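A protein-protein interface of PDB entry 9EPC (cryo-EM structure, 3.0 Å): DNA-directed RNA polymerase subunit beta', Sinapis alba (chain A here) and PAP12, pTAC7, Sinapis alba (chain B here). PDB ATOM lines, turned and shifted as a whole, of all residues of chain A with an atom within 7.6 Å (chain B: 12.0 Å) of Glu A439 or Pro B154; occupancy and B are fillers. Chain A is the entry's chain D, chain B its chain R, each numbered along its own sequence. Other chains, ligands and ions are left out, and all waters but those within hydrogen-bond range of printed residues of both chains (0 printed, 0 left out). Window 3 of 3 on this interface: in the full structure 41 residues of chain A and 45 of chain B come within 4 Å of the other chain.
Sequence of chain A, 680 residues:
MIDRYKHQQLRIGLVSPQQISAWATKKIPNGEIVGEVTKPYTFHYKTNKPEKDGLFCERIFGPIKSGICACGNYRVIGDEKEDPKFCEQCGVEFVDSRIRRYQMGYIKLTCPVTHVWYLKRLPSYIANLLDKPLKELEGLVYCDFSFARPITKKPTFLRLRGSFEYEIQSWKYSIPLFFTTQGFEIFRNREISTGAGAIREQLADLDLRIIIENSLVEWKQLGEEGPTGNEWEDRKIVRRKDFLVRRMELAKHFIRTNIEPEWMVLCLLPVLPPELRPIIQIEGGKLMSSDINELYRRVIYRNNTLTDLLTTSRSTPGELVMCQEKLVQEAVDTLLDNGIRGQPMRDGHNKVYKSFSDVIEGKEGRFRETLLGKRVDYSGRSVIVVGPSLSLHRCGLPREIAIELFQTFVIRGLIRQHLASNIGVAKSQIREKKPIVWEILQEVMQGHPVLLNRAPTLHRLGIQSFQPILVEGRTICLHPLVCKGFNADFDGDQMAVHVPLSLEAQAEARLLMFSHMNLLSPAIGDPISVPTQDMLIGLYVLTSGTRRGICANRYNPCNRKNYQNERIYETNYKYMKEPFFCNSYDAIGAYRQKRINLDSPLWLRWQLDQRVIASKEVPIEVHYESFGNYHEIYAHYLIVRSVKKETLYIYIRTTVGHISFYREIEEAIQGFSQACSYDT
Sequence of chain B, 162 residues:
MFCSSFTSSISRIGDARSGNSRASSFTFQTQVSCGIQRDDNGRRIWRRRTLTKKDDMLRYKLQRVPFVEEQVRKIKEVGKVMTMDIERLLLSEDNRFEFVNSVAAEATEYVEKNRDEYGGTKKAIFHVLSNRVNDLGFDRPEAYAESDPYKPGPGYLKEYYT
The backbone carbonyl oxygen (O) of Val A444 sits at hydrogen-bond distance from the side-chain amino group (NZ) of Lys B123 (3.5 Å). O of Glu A443 sits close to O of Gly B120 (3.3 Å). The side-chain carboxylate of Glu A439 lies close to the backbone carbonyl oxygen of Pro B154, at 3.0 Å.
OE2 of Glu A443 is in hydrogen-bond range of NE2 of Gln A417, at 2.8 Å.
Among the printed residues, pairs that only touch across the chains: Arg A399 with Leu B157 (3.3 Å), Glu A443 with Thr B121 (3.8 Å) and Trp A438 with Leu B157 (3.9 Å).
Of chain B, only Pro B154 (3.0 Å) comes within 4 Å of Glu A439. Of chain A, only Glu A439 comes within 4 Å of Pro B154. No residue of chain B comes within 4 Å of Val A437. No residue of chain B comes within 4 Å of Ile A440. Glu A443 touches just these residues of chain B: Gly B120 and Thr B121. Of the printed residues of chain B, Arg A399 touches Leu B157. Of the printed residues of chain A, Lys B123 touches Val A444. Of the printed residues of chain A, Gly B120 touches Glu A443 (3.3 Å). Of the printed residues of chain B, Trp A438 touches Leu B157. Of the printed residues of chain A, Thr B121 touches Glu A443. Pro A435 touches none of the printed residues of chain B.
Printed residues of chain B that touch a printed residue of chain A: Gly B120, Thr B121, Lys B123, Pro B154 and Leu B157. Hydrophobic or aromatic side chains of chain A that line the printed part of chain B: Trp A438.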
ATOM      1  N   ARG A 399       7.889  29.945 -29.651  1.00  0.00           N
ATOM      2  CA  ARG A 399       6.864  28.916 -29.516  1.00  0.00           C
ATOM      3  C   ARG A 399       7.091  27.771 -30.494  1.00  0.00           C
ATOM      4  O   ARG A 399       6.957  26.599 -30.126  1.00  0.00           O
ATOM      5  CB  ARG A 399       5.477  29.520 -29.719  1.00  0.00           C
ATOM      6  CG  ARG A 399       5.037  30.441 -28.601  1.00  0.00           C
ATOM      7  CD  ARG A 399       3.554  30.731 -28.700  1.00  0.00           C
ATOM      8  NE  ARG A 399       3.093  31.600 -27.624  1.00  0.00           N
ATOM      9  CZ  ARG A 399       1.825  31.921 -27.418  1.00  0.00           C
ATOM     10  NH1 ARG A 399       0.858  31.452 -28.189  1.00  0.00           N
ATOM     11  NH2 ARG A 399       1.518  32.735 -26.411  1.00  0.00           N
ATOM     12  N   VAL A 410       5.103  17.699 -23.882  1.00  0.00           N
ATOM     13  CA  VAL A 410       3.775  18.284 -24.036  1.00  0.00           C
ATOM     14  C   VAL A 410       2.726  17.192 -24.184  1.00  0.00           C
ATOM     15  O   VAL A 410       1.646  17.262 -23.584  1.00  0.00           O
ATOM     16  CB  VAL A 410       3.753  19.259 -25.226  1.00  0.00           C
ATOM     17  CG1 VAL A 410       2.327  19.650 -25.561  1.00  0.00           C
ATOM     18  CG2 VAL A 410       4.567  20.493 -24.905  1.00  0.00           C
ATOM     19  N   LEU A 414      -0.605  16.494 -21.790  1.00  0.00           N
ATOM     20  CA  LEU A 414      -1.980  16.358 -22.258  1.00  0.00           C
ATOM     21  C   LEU A 414      -2.595  15.046 -21.787  1.00  0.00           C
ATOM     22  O   LEU A 414      -3.753  15.012 -21.357  1.00  0.00           O
ATOM     23  CB  LEU A 414      -2.028  16.457 -23.781  1.00  0.00           C
ATOM     24  CG  LEU A 414      -1.588  17.793 -24.378  1.00  0.00           C
ATOM     25  CD1 LEU A 414      -1.624  17.740 -25.894  1.00  0.00           C
ATOM     26  CD2 LEU A 414      -2.466  18.916 -23.858  1.00  0.00           C
ATOM     27  N   GLN A 417      -3.143  15.094 -17.803  1.00  0.00           N
ATOM     28  CA  GLN A 417      -4.285  15.884 -17.369  1.00  0.00           C
ATOM     29  C   GLN A 417      -5.563  15.529 -18.116  1.00  0.00           C
ATOM     30  O   GLN A 417      -6.540  16.280 -18.041  1.00  0.00           O
ATOM     31  CB  GLN A 417      -3.977  17.375 -17.520  1.00  0.00           C
ATOM     32  CG  GLN A 417      -2.771  17.830 -16.716  1.00  0.00           C
ATOM     33  CD  GLN A 417      -2.519  19.319 -16.825  1.00  0.00           C
ATOM     34  OE1 GLN A 417      -3.316  20.056 -17.404  1.00  0.00           O
ATOM     35  NE2 GLN A 417      -1.403  19.773 -16.265  1.00  0.00           N
ATOM     36  N   LYS A 434      -4.148  24.127 -30.244  1.00  0.00           N
ATOM     37  CA  LYS A 434      -5.154  24.584 -29.303  1.00  0.00           C
ATOM     38  C   LYS A 434      -4.521  25.504 -28.261  1.00  0.00           C
ATOM     39  O   LYS A 434      -3.326  25.399 -27.971  1.00  0.00           O
ATOM     40  CB  LYS A 434      -5.814  23.397 -28.609  1.00  0.00           C
ATOM     41  CG  LYS A 434      -6.447  22.389 -29.552  1.00  0.00           C
ATOM     42  CD  LYS A 434      -7.598  23.000 -30.330  1.00  0.00           C
ATOM     43  CE  LYS A 434      -8.293  21.956 -31.185  1.00  0.00           C
ATOM     44  NZ  LYS A 434      -9.381  22.549 -32.008  1.00  0.00           N
ATOM     45  N   PRO A 435      -5.299  26.428 -27.693  1.00  0.00           N
ATOM     46  CA  PRO A 435      -4.748  27.291 -26.634  1.00  0.00           C
ATOM     47  C   PRO A 435      -4.266  26.518 -25.421  1.00  0.00           C
ATOM     48  O   PRO A 435      -3.363  26.987 -24.716  1.00  0.00           O
ATOM     49  CB  PRO A 435      -5.927  28.212 -26.288  1.00  0.00           C
ATOM     50  CG  PRO A 435      -6.789  28.197 -27.505  1.00  0.00           C
ATOM     51  CD  PRO A 435      -6.671  26.813 -28.062  1.00  0.00           C
ATOM     52  N   ILE A 436      -4.847  25.347 -25.149  1.00  0.00           N
ATOM     53  CA  ILE A 436      -4.400  24.537 -24.021  1.00  0.00           C
ATOM     54  C   ILE A 436      -2.985  24.021 -24.252  1.00  0.00           C
ATOM     55  O   ILE A 436      -2.208  23.877 -23.300  1.00  0.00           O
ATOM     56  CB  ILE A 436      -5.394  23.389 -23.768  1.00  0.00           C
ATOM     57  CG1 ILE A 436      -4.907  22.486 -22.633  1.00  0.00           C
ATOM     58  CG2 ILE A 436      -5.623  22.586 -25.039  1.00  0.00           C
ATOM     59  CD1 ILE A 436      -4.759  23.198 -21.310  1.00  0.00           C
ATOM     60  N   VAL A 437      -2.624  23.745 -25.507  1.00  0.00           N
ATOM     61  CA  VAL A 437      -1.306  23.191 -25.803  1.00  0.00           C
ATOM     62  C   VAL A 437      -0.209  24.144 -25.350  1.00  0.00           C
ATOM     63  O   VAL A 437       0.785  23.726 -24.744  1.00  0.00           O
ATOM     64  CB  VAL A 437      -1.189  22.868 -27.304  1.00  0.00           C
ATOM     65  CG1 VAL A 437       0.191  22.321 -27.621  1.00  0.00           C
ATOM     66  CG2 VAL A 437      -2.264  21.880 -27.715  1.00  0.00           C
ATOM     67  N   TRP A 438      -0.370  25.437 -25.632  1.00  0.00           N
ATOM     68  CA  TRP A 438       0.629  26.409 -25.203  1.00  0.00           C
ATOM     69  C   TRP A 438       0.679  26.533 -23.688  1.00  0.00           C
ATOM     70  O   TRP A 438       1.758  26.735 -23.120  1.00  0.00           O
ATOM     71  CB  TRP A 438       0.352  27.766 -25.845  1.00  0.00           C
ATOM     72  CG  TRP A 438       0.282  27.694 -27.329  1.00  0.00           C
ATOM     73  CD1 TRP A 438      -0.798  27.968 -28.111  1.00  0.00           C
ATOM     74  CD2 TRP A 438       1.332  27.301 -28.218  1.00  0.00           C
ATOM     75  NE1 TRP A 438      -0.485  27.781 -29.434  1.00  0.00           N
ATOM     76  CE2 TRP A 438       0.818  27.371 -29.527  1.00  0.00           C
ATOM     77  CE3 TRP A 438       2.658  26.902 -28.036  1.00  0.00           C
ATOM     78  CZ2 TRP A 438       1.584  27.056 -30.645  1.00  0.00           C
ATOM     79  CZ3 TRP A 438       3.415  26.590 -29.147  1.00  0.00           C
ATOM     80  CH2 TRP A 438       2.876  26.669 -30.435  1.00  0.00           C
ATOM     81  N   GLU A 439      -0.469  26.425 -23.017  1.00  0.00           N
ATOM     82  CA  GLU A 439      -0.466  26.440 -21.559  1.00  0.00           C
ATOM     83  C   GLU A 439       0.269  25.229 -21.000  1.00  0.00           C
ATOM     84  O   GLU A 439       1.023  25.345 -20.028  1.00  0.00           O
ATOM     85  CB  GLU A 439      -1.898  26.493 -21.031  1.00  0.00           C
ATOM     86  CG  GLU A 439      -1.993  26.564 -19.519  1.00  0.00           C
ATOM     87  CD  GLU A 439      -3.417  26.735 -19.032  1.00  0.00           C
ATOM     88  OE1 GLU A 439      -4.320  26.904 -19.878  1.00  0.00           O
ATOM     89  OE2 GLU A 439      -3.633  26.700 -17.802  1.00  0.00           O
ATOM     90  N   ILE A 440       0.058  24.057 -21.601  1.00  0.00           N
ATOM     91  CA  ILE A 440       0.790  22.865 -21.186  1.00  0.00           C
ATOM     92  C   ILE A 440       2.276  23.029 -21.473  1.00  0.00           C
ATOM     93  O   ILE A 440       3.126  22.663 -20.653  1.00  0.00           O
ATOM     94  CB  ILE A 440       0.213  21.617 -21.875  1.00  0.00           C
ATOM     95  CG1 ILE A 440      -1.226  21.381 -21.420  1.00  0.00           C
ATOM     96  CG2 ILE A 440       1.070  20.399 -21.582  1.00  0.00           C
ATOM     97  CD1 ILE A 440      -1.370  21.211 -19.926  1.00  0.00           C
ATOM     98  N   LEU A 441       2.615  23.578 -22.641  1.00  0.00           N
ATOM     99  CA  LEU A 441       4.018  23.796 -22.974  1.00  0.00           C
ATOM    100  C   LEU A 441       4.671  24.764 -21.997  1.00  0.00           C
ATOM    101  O   LEU A 441       5.829  24.578 -21.609  1.00  0.00           O
ATOM    102  CB  LEU A 441       4.139  24.314 -24.405  1.00  0.00           C
ATOM    103  CG  LEU A 441       5.530  24.753 -24.862  1.00  0.00           C
ATOM    104  CD1 LEU A 441       6.511  23.601 -24.780  1.00  0.00           C
ATOM    105  CD2 LEU A 441       5.472  25.304 -26.274  1.00  0.00           C
ATOM    106  N   GLN A 442       3.940  25.802 -21.586  1.00  0.00           N
ATOM    107  CA  GLN A 442       4.506  26.786 -20.670  1.00  0.00           C
ATOM    108  C   GLN A 442       4.865  26.154 -19.331  1.00  0.00           C
ATOM    109  O   GLN A 442       5.931  26.434 -18.771  1.00  0.00           O
ATOM    110  CB  GLN A 442       3.526  27.943 -20.479  1.00  0.00           C
ATOM    111  CG  GLN A 442       4.075  29.116 -19.683  1.00  0.00           C
ATOM    112  CD  GLN A 442       3.893  28.947 -18.187  1.00  0.00           C
ATOM    113  OE1 GLN A 442       3.101  28.120 -17.735  1.00  0.00           O
ATOM    114  NE2 GLN A 442       4.631  29.731 -17.410  1.00  0.00           N
ATOM    115  N   GLU A 443       3.989  25.300 -18.798  1.00  0.00           N
ATOM    116  CA  GLU A 443       4.280  24.652 -17.524  1.00  0.00           C
ATOM    117  C   GLU A 443       5.281  23.515 -17.677  1.00  0.00           C
ATOM    118  O   GLU A 443       5.971  23.171 -16.711  1.00  0.00           O
ATOM    119  CB  GLU A 443       2.993  24.134 -16.885  1.00  0.00           C
ATOM    120  CG  GLU A 443       2.387  22.936 -17.584  1.00  0.00           C
ATOM    121  CD  GLU A 443       1.131  22.438 -16.902  1.00  0.00           C
ATOM    122  OE1 GLU A 443       0.561  23.192 -16.086  1.00  0.00           O
ATOM    123  OE2 GLU A 443       0.716  21.294 -17.179  1.00  0.00           O
ATOM    124  N   VAL A 444       5.370  22.919 -18.866  1.00  0.00           N
ATOM    125  CA  VAL A 444       6.310  21.825 -19.081  1.00  0.00           C
ATOM    126  C   VAL A 444       7.745  22.334 -19.036  1.00  0.00           C
ATOM    127  O   VAL A 444       8.609  21.745 -18.377  1.00  0.00           O
ATOM    128  CB  VAL A 444       6.001  21.111 -20.409  1.00  0.00           C
ATOM    129  CG1 VAL A 444       7.266  20.537 -21.010  1.00  0.00           C
ATOM    130  CG2 VAL A 444       4.979  20.015 -20.185  1.00  0.00           C
ATOM    131  N   MET A 445       8.020  23.440 -19.732  1.00  0.00           N
ATOM    132  CA  MET A 445       9.380  23.967 -19.756  1.00  0.00           C
ATOM    133  C   MET A 445       9.791  24.512 -18.399  1.00  0.00           C
ATOM    134  O   MET A 445      10.989  24.593 -18.103  1.00  0.00           O
ATOM    135  CB  MET A 445       9.508  25.060 -20.813  1.00  0.00           C
ATOM    136  CG  MET A 445       8.960  24.690 -22.170  1.00  0.00           C
ATOM    137  SD  MET A 445       9.387  25.940 -23.389  1.00  0.00           S
ATOM    138  CE  MET A 445       9.158  27.421 -22.420  1.00  0.00           C
ATOM    139  N   LEU A 470       9.119  30.675 -22.304  1.00  0.00           N
ATOM    140  CA  LEU A 470       8.419  30.849 -23.569  1.00  0.00           C
ATOM    141  C   LEU A 470       8.308  32.332 -23.884  1.00  0.00           C
ATOM    142  O   LEU A 470       7.738  33.100 -23.102  1.00  0.00           O
ATOM    143  CB  LEU A 470       7.040  30.202 -23.499  1.00  0.00           C
ATOM    144  CG  LEU A 470       6.325  29.990 -24.831  1.00  0.00           C
ATOM    145  CD1 LEU A 470       7.174  29.137 -25.753  1.00  0.00           C
ATOM    146  CD2 LEU A 470       4.972  29.347 -24.599  1.00  0.00           C
ATOM    147  N   GLY B 119       4.984  16.118 -13.410  1.00  0.00           N
ATOM    148  CA  GLY B 119       4.946  16.321 -14.844  1.00  0.00           C
ATOM    149  C   GLY B 119       4.843  17.769 -15.274  1.00  0.00           C
ATOM    150  O   GLY B 119       5.367  18.148 -16.323  1.00  0.00           O
ATOM    151  N   GLY B 120       4.182  18.591 -14.465  1.00  0.00           N
ATOM    152  CA  GLY B 120       3.893  19.953 -14.865  1.00  0.00           C
ATOM    153  C   GLY B 120       4.506  21.008 -13.973  1.00  0.00           C
ATOM    154  O   GLY B 120       5.717  21.240 -14.011  1.00  0.00           O
ATOM    155  N   THR B 121       3.666  21.662 -13.167  1.00  0.00           N
ATOM    156  CA  THR B 121       4.145  22.719 -12.284  1.00  0.00           C
ATOM    157  C   THR B 121       5.133  22.205 -11.250  1.00  0.00           C
ATOM    158  O   THR B 121       5.940  22.986 -10.736  1.00  0.00           O
ATOM    159  CB  THR B 121       2.967  23.391 -11.579  1.00  0.00           C
ATOM    160  OG1 THR B 121       2.323  22.445 -10.718  1.00  0.00           O
ATOM    161  CG2 THR B 121       1.963  23.904 -12.598  1.00  0.00           C
ATOM    162  N   LYS B 122       5.091  20.915 -10.935  1.00  0.00           N
ATOM    163  CA  LYS B 122       6.010  20.305  -9.987  1.00  0.00           C
ATOM    164  C   LYS B 122       6.991  19.420 -10.741  1.00  0.00           C
ATOM    165  O   LYS B 122       6.582  18.581 -11.548  1.00  0.00           O
ATOM    166  CB  LYS B 122       5.255  19.486  -8.939  1.00  0.00           C
ATOM    167  CG  LYS B 122       6.150  18.826  -7.913  1.00  0.00           C
ATOM    168  CD  LYS B 122       5.334  18.066  -6.888  1.00  0.00           C
ATOM    169  CE  LYS B 122       4.337  18.978  -6.201  1.00  0.00           C
ATOM    170  NZ  LYS B 122       3.522  18.241  -5.199  1.00  0.00           N
ATOM    171  N   LYS B 123       8.277  19.617 -10.483  1.00  0.00           N
ATOM    172  CA  LYS B 123       9.332  18.831 -11.097  1.00  0.00           C
ATOM    173  C   LYS B 123       9.972  17.934 -10.047  1.00  0.00           C
ATOM    174  O   LYS B 123      10.104  18.313  -8.880  1.00  0.00           O
ATOM    175  CB  LYS B 123      10.393  19.732 -11.732  1.00  0.00           C
ATOM    176  CG  LYS B 123       9.817  20.873 -12.553  1.00  0.00           C
ATOM    177  CD  LYS B 123       9.040  20.363 -13.752  1.00  0.00           C
ATOM    178  CE  LYS B 123       9.954  19.666 -14.739  1.00  0.00           C
ATOM    179  NZ  LYS B 123       9.236  19.299 -15.987  1.00  0.00           N
ATOM    180  N   GLU B 146       5.533  28.046  -8.202  1.00  0.00           N
ATOM    181  CA  GLU B 146       4.815  29.290  -7.977  1.00  0.00           C
ATOM    182  C   GLU B 146       3.729  29.445  -9.030  1.00  0.00           C
ATOM    183  O   GLU B 146       3.935  29.113 -10.200  1.00  0.00           O
ATOM    184  CB  GLU B 146       5.756  30.498  -8.022  1.00  0.00           C
ATOM    185  CG  GLU B 146       5.092  31.810  -7.640  1.00  0.00           C
ATOM    186  CD  GLU B 146       5.867  33.017  -8.123  1.00  0.00           C
ATOM    187  OE1 GLU B 146       6.764  32.846  -8.974  1.00  0.00           O
ATOM    188  OE2 GLU B 146       5.578  34.137  -7.654  1.00  0.00           O
ATOM    189  N   SER B 147       2.577  29.953  -8.606  1.00  0.00           N
ATOM    190  CA  SER B 147       1.470  30.232  -9.503  1.00  0.00           C
ATOM    191  C   SER B 147       1.496  31.703  -9.909  1.00  0.00           C
ATOM    192  O   SER B 147       2.371  32.474  -9.507  1.00  0.00           O
ATOM    193  CB  SER B 147       0.140  29.866  -8.841  1.00  0.00           C
ATOM    194  OG  SER B 147      -0.059  30.616  -7.655  1.00  0.00           O
ATOM    195  N   ASP B 148       0.514  32.098 -10.719  1.00  0.00           N
ATOM    196  CA  ASP B 148       0.368  33.480 -11.167  1.00  0.00           C
ATOM    197  C   ASP B 148      -0.933  34.031 -10.601  1.00  0.00           C
ATOM    198  O   ASP B 148      -2.006  33.840 -11.192  1.00  0.00           O
ATOM    199  CB  ASP B 148       0.379  33.565 -12.695  1.00  0.00           C
ATOM    200  CG  ASP B 148       0.471  34.990 -13.199  1.00  0.00           C
ATOM    201  OD1 ASP B 148       0.676  35.903 -12.372  1.00  0.00           O
ATOM    202  OD2 ASP B 148       0.339  35.199 -14.422  1.00  0.00           O
ATOM    203  N   PRO B 149      -0.896  34.721  -9.459  1.00  0.00           N
ATOM    204  CA  PRO B 149      -2.145  35.216  -8.858  1.00  0.00           C
ATOM    205  C   PRO B 149      -2.858  36.255  -9.699  1.00  0.00           C
ATOM    206  O   PRO B 149      -4.057  36.479  -9.493  1.00  0.00           O
ATOM    207  CB  PRO B 149      -1.678  35.803  -7.519  1.00  0.00           C
ATOM    208  CG  PRO B 149      -0.241  36.138  -7.738  1.00  0.00           C
ATOM    209  CD  PRO B 149       0.289  35.092  -8.669  1.00  0.00           C
ATOM    210  N   TYR B 150      -2.168  36.896 -10.639  1.00  0.00           N
ATOM    211  CA  TYR B 150      -2.749  37.946 -11.459  1.00  0.00           C
ATOM    212  C   TYR B 150      -3.135  37.461 -12.848  1.00  0.00           C
ATOM    213  O   TYR B 150      -3.427  38.282 -13.722  1.00  0.00           O
ATOM    214  CB  TYR B 150      -1.779  39.122 -11.558  1.00  0.00           C
ATOM    215  CG  TYR B 150      -1.144  39.461 -10.234  1.00  0.00           C
ATOM    216  CD1 TYR B 150      -1.886  40.049  -9.219  1.00  0.00           C
ATOM    217  CD2 TYR B 150       0.192  39.180  -9.989  1.00  0.00           C
ATOM    218  CE1 TYR B 150      -1.313  40.355  -8.004  1.00  0.00           C
ATOM    219  CE2 TYR B 150       0.774  39.483  -8.776  1.00  0.00           C
ATOM    220  CZ  TYR B 150       0.016  40.071  -7.787  1.00  0.00           C
ATOM    221  OH  TYR B 150       0.591  40.376  -6.575  1.00  0.00           O
ATOM    222  N   LYS B 151      -3.144  36.156 -13.069  1.00  0.00           N
ATOM    223  CA  LYS B 151      -3.534  35.616 -14.363  1.00  0.00           C
ATOM    224  C   LYS B 151      -5.021  35.854 -14.580  1.00  0.00           C
ATOM    225  O   LYS B 151      -5.836  35.396 -13.768  1.00  0.00           O
ATOM    226  CB  LYS B 151      -3.201  34.129 -14.421  1.00  0.00           C
ATOM    227  CG  LYS B 151      -3.543  33.440 -15.726  1.00  0.00           C
ATOM    228  CD  LYS B 151      -2.846  32.090 -15.803  1.00  0.00           C
ATOM    229  CE  LYS B 151      -3.516  31.165 -16.801  1.00  0.00           C
ATOM    230  NZ  LYS B 151      -4.883  30.787 -16.358  1.00  0.00           N
ATOM    231  N   PRO B 152      -5.420  36.564 -15.634  1.00  0.00           N
ATOM    232  CA  PRO B 152      -6.836  36.921 -15.795  1.00  0.00           C
ATOM    233  C   PRO B 152      -7.741  35.737 -16.099  1.00  0.00           C
ATOM    234  O   PRO B 152      -8.760  35.543 -15.428  1.00  0.00           O
ATOM    235  CB  PRO B 152      -6.812  37.917 -16.961  1.00  0.00           C
ATOM    236  CG  PRO B 152      -5.577  37.582 -17.717  1.00  0.00           C
ATOM    237  CD  PRO B 152      -4.577  37.127 -16.701  1.00  0.00           C
ATOM    238  N   GLY B 153      -7.385  34.938 -17.101  1.00  0.00           N
ATOM    239  CA  GLY B 153      -8.232  33.857 -17.538  1.00  0.00           C
ATOM    240  C   GLY B 153      -7.462  32.595 -17.867  1.00  0.00           C
ATOM    241  O   GLY B 153      -6.235  32.605 -18.002  1.00  0.00           O
ATOM    242  N   PRO B 154      -8.178  31.474 -17.991  1.00  0.00           N
ATOM    243  CA  PRO B 154      -7.497  30.208 -18.307  1.00  0.00           C
ATOM    244  C   PRO B 154      -6.762  30.229 -19.636  1.00  0.00           C
ATOM    245  O   PRO B 154      -5.691  29.622 -19.755  1.00  0.00           O
ATOM    246  CB  PRO B 154      -8.647  29.189 -18.305  1.00  0.00           C
ATOM    247  CG  PRO B 154      -9.868  29.999 -18.593  1.00  0.00           C
ATOM    248  CD  PRO B 154      -9.641  31.320 -17.923  1.00  0.00           C
ATOM    249  N   GLY B 155      -7.303  30.917 -20.639  1.00  0.00           N
ATOM    250  CA  GLY B 155      -6.650  30.979 -21.932  1.00  0.00           C
ATOM    251  C   GLY B 155      -5.556  32.015 -22.050  1.00  0.00           C
ATOM    252  O   GLY B 155      -4.833  32.024 -23.051  1.00  0.00           O
ATOM    253  N   TYR B 156      -5.411  32.882 -21.052  1.00  0.00           N
ATOM    254  CA  TYR B 156      -4.413  33.945 -21.078  1.00  0.00           C
ATOM    255  C   TYR B 156      -3.115  33.420 -20.481  1.00  0.00           C
ATOM    256  O   TYR B 156      -3.057  33.089 -19.292  1.00  0.00           O
ATOM    257  CB  TYR B 156      -4.910  35.168 -20.312  1.00  0.00           C
ATOM    258  CG  TYR B 156      -6.035  35.906 -20.995  1.00  0.00           C
ATOM    259  CD1 TYR B 156      -7.356  35.532 -20.800  1.00  0.00           C
ATOM    260  CD2 TYR B 156      -5.775  36.980 -21.835  1.00  0.00           C
ATOM    261  CE1 TYR B 156      -8.386  36.206 -21.423  1.00  0.00           C
ATOM    262  CE2 TYR B 156      -6.798  37.659 -22.462  1.00  0.00           C
ATOM    263  CZ  TYR B 156      -8.102  37.268 -22.253  1.00  0.00           C
ATOM    264  OH  TYR B 156      -9.124  37.944 -22.877  1.00  0.00           O
ATOM    265  N   LEU B 157      -2.073  33.346 -21.302  1.00  0.00           N
ATOM    266  CA  LEU B 157      -0.745  32.961 -20.852  1.00  0.00           C
ATOM    267  C   LEU B 157       0.165  34.182 -20.886  1.00  0.00           C
ATOM    268  O   LEU B 157       0.110  34.984 -21.824  1.00  0.00           O
ATOM    269  CB  LEU B 157      -0.163  31.830 -21.709  1.00  0.00           C
ATOM    270  CG  LEU B 157       0.183  32.052 -23.183  1.00  0.00           C
ATOM    271  CD1 LEU B 157       1.119  30.954 -23.653  1.00  0.00           C
ATOM    272  CD2 LEU B 157      -1.062  32.085 -24.054  1.00  0.00           C
ATOM    273  N   LYS B 158       0.993  34.319 -19.855  1.00  0.00           N
ATOM    274  CA  LYS B 158       1.780  35.531 -19.652  1.00  0.00           C
ATOM    275  C   LYS B 158       2.807  35.681 -20.766  1.00  0.00           C
ATOM    276  O   LYS B 158       3.797  34.946 -20.813  1.00  0.00           O
ATOM    277  CB  LYS B 158       2.462  35.487 -18.288  1.00  0.00           C
ATOM    278  CG  LYS B 158       3.203  36.760 -17.923  1.00  0.00           C
ATOM    279  CD  LYS B 158       3.922  36.616 -16.594  1.00  0.00           C
ATOM    280  CE  LYS B 158       4.539  37.930 -16.151  1.00  0.00           C
ATOM    281  NZ  LYS B 158       5.477  38.479 -17.166  1.00  0.00           N
ATOM    282  N   GLU B 159       2.571  36.632 -21.664  1.00  0.00           N
ATOM    283  CA  GLU B 159       3.569  36.986 -22.661  1.00  0.00           C
ATOM    284  C   GLU B 159       4.776  37.621 -21.984  1.00  0.00           C
ATOM    285  O   GLU B 159       4.634  38.456 -21.087  1.00  0.00           O
ATOM    286  CB  GLU B 159       2.974  37.944 -23.691  1.00  0.00           C
ATOM    287  CG  GLU B 159       3.964  38.953 -24.250  1.00  0.00           C
ATOM    288  CD  GLU B 159       3.333  39.909 -25.242  1.00  0.00           C
ATOM    289  OE1 GLU B 159       2.159  39.694 -25.613  1.00  0.00           O
ATOM    290  OE2 GLU B 159       4.009  40.877 -25.650  1.00  0.00           O
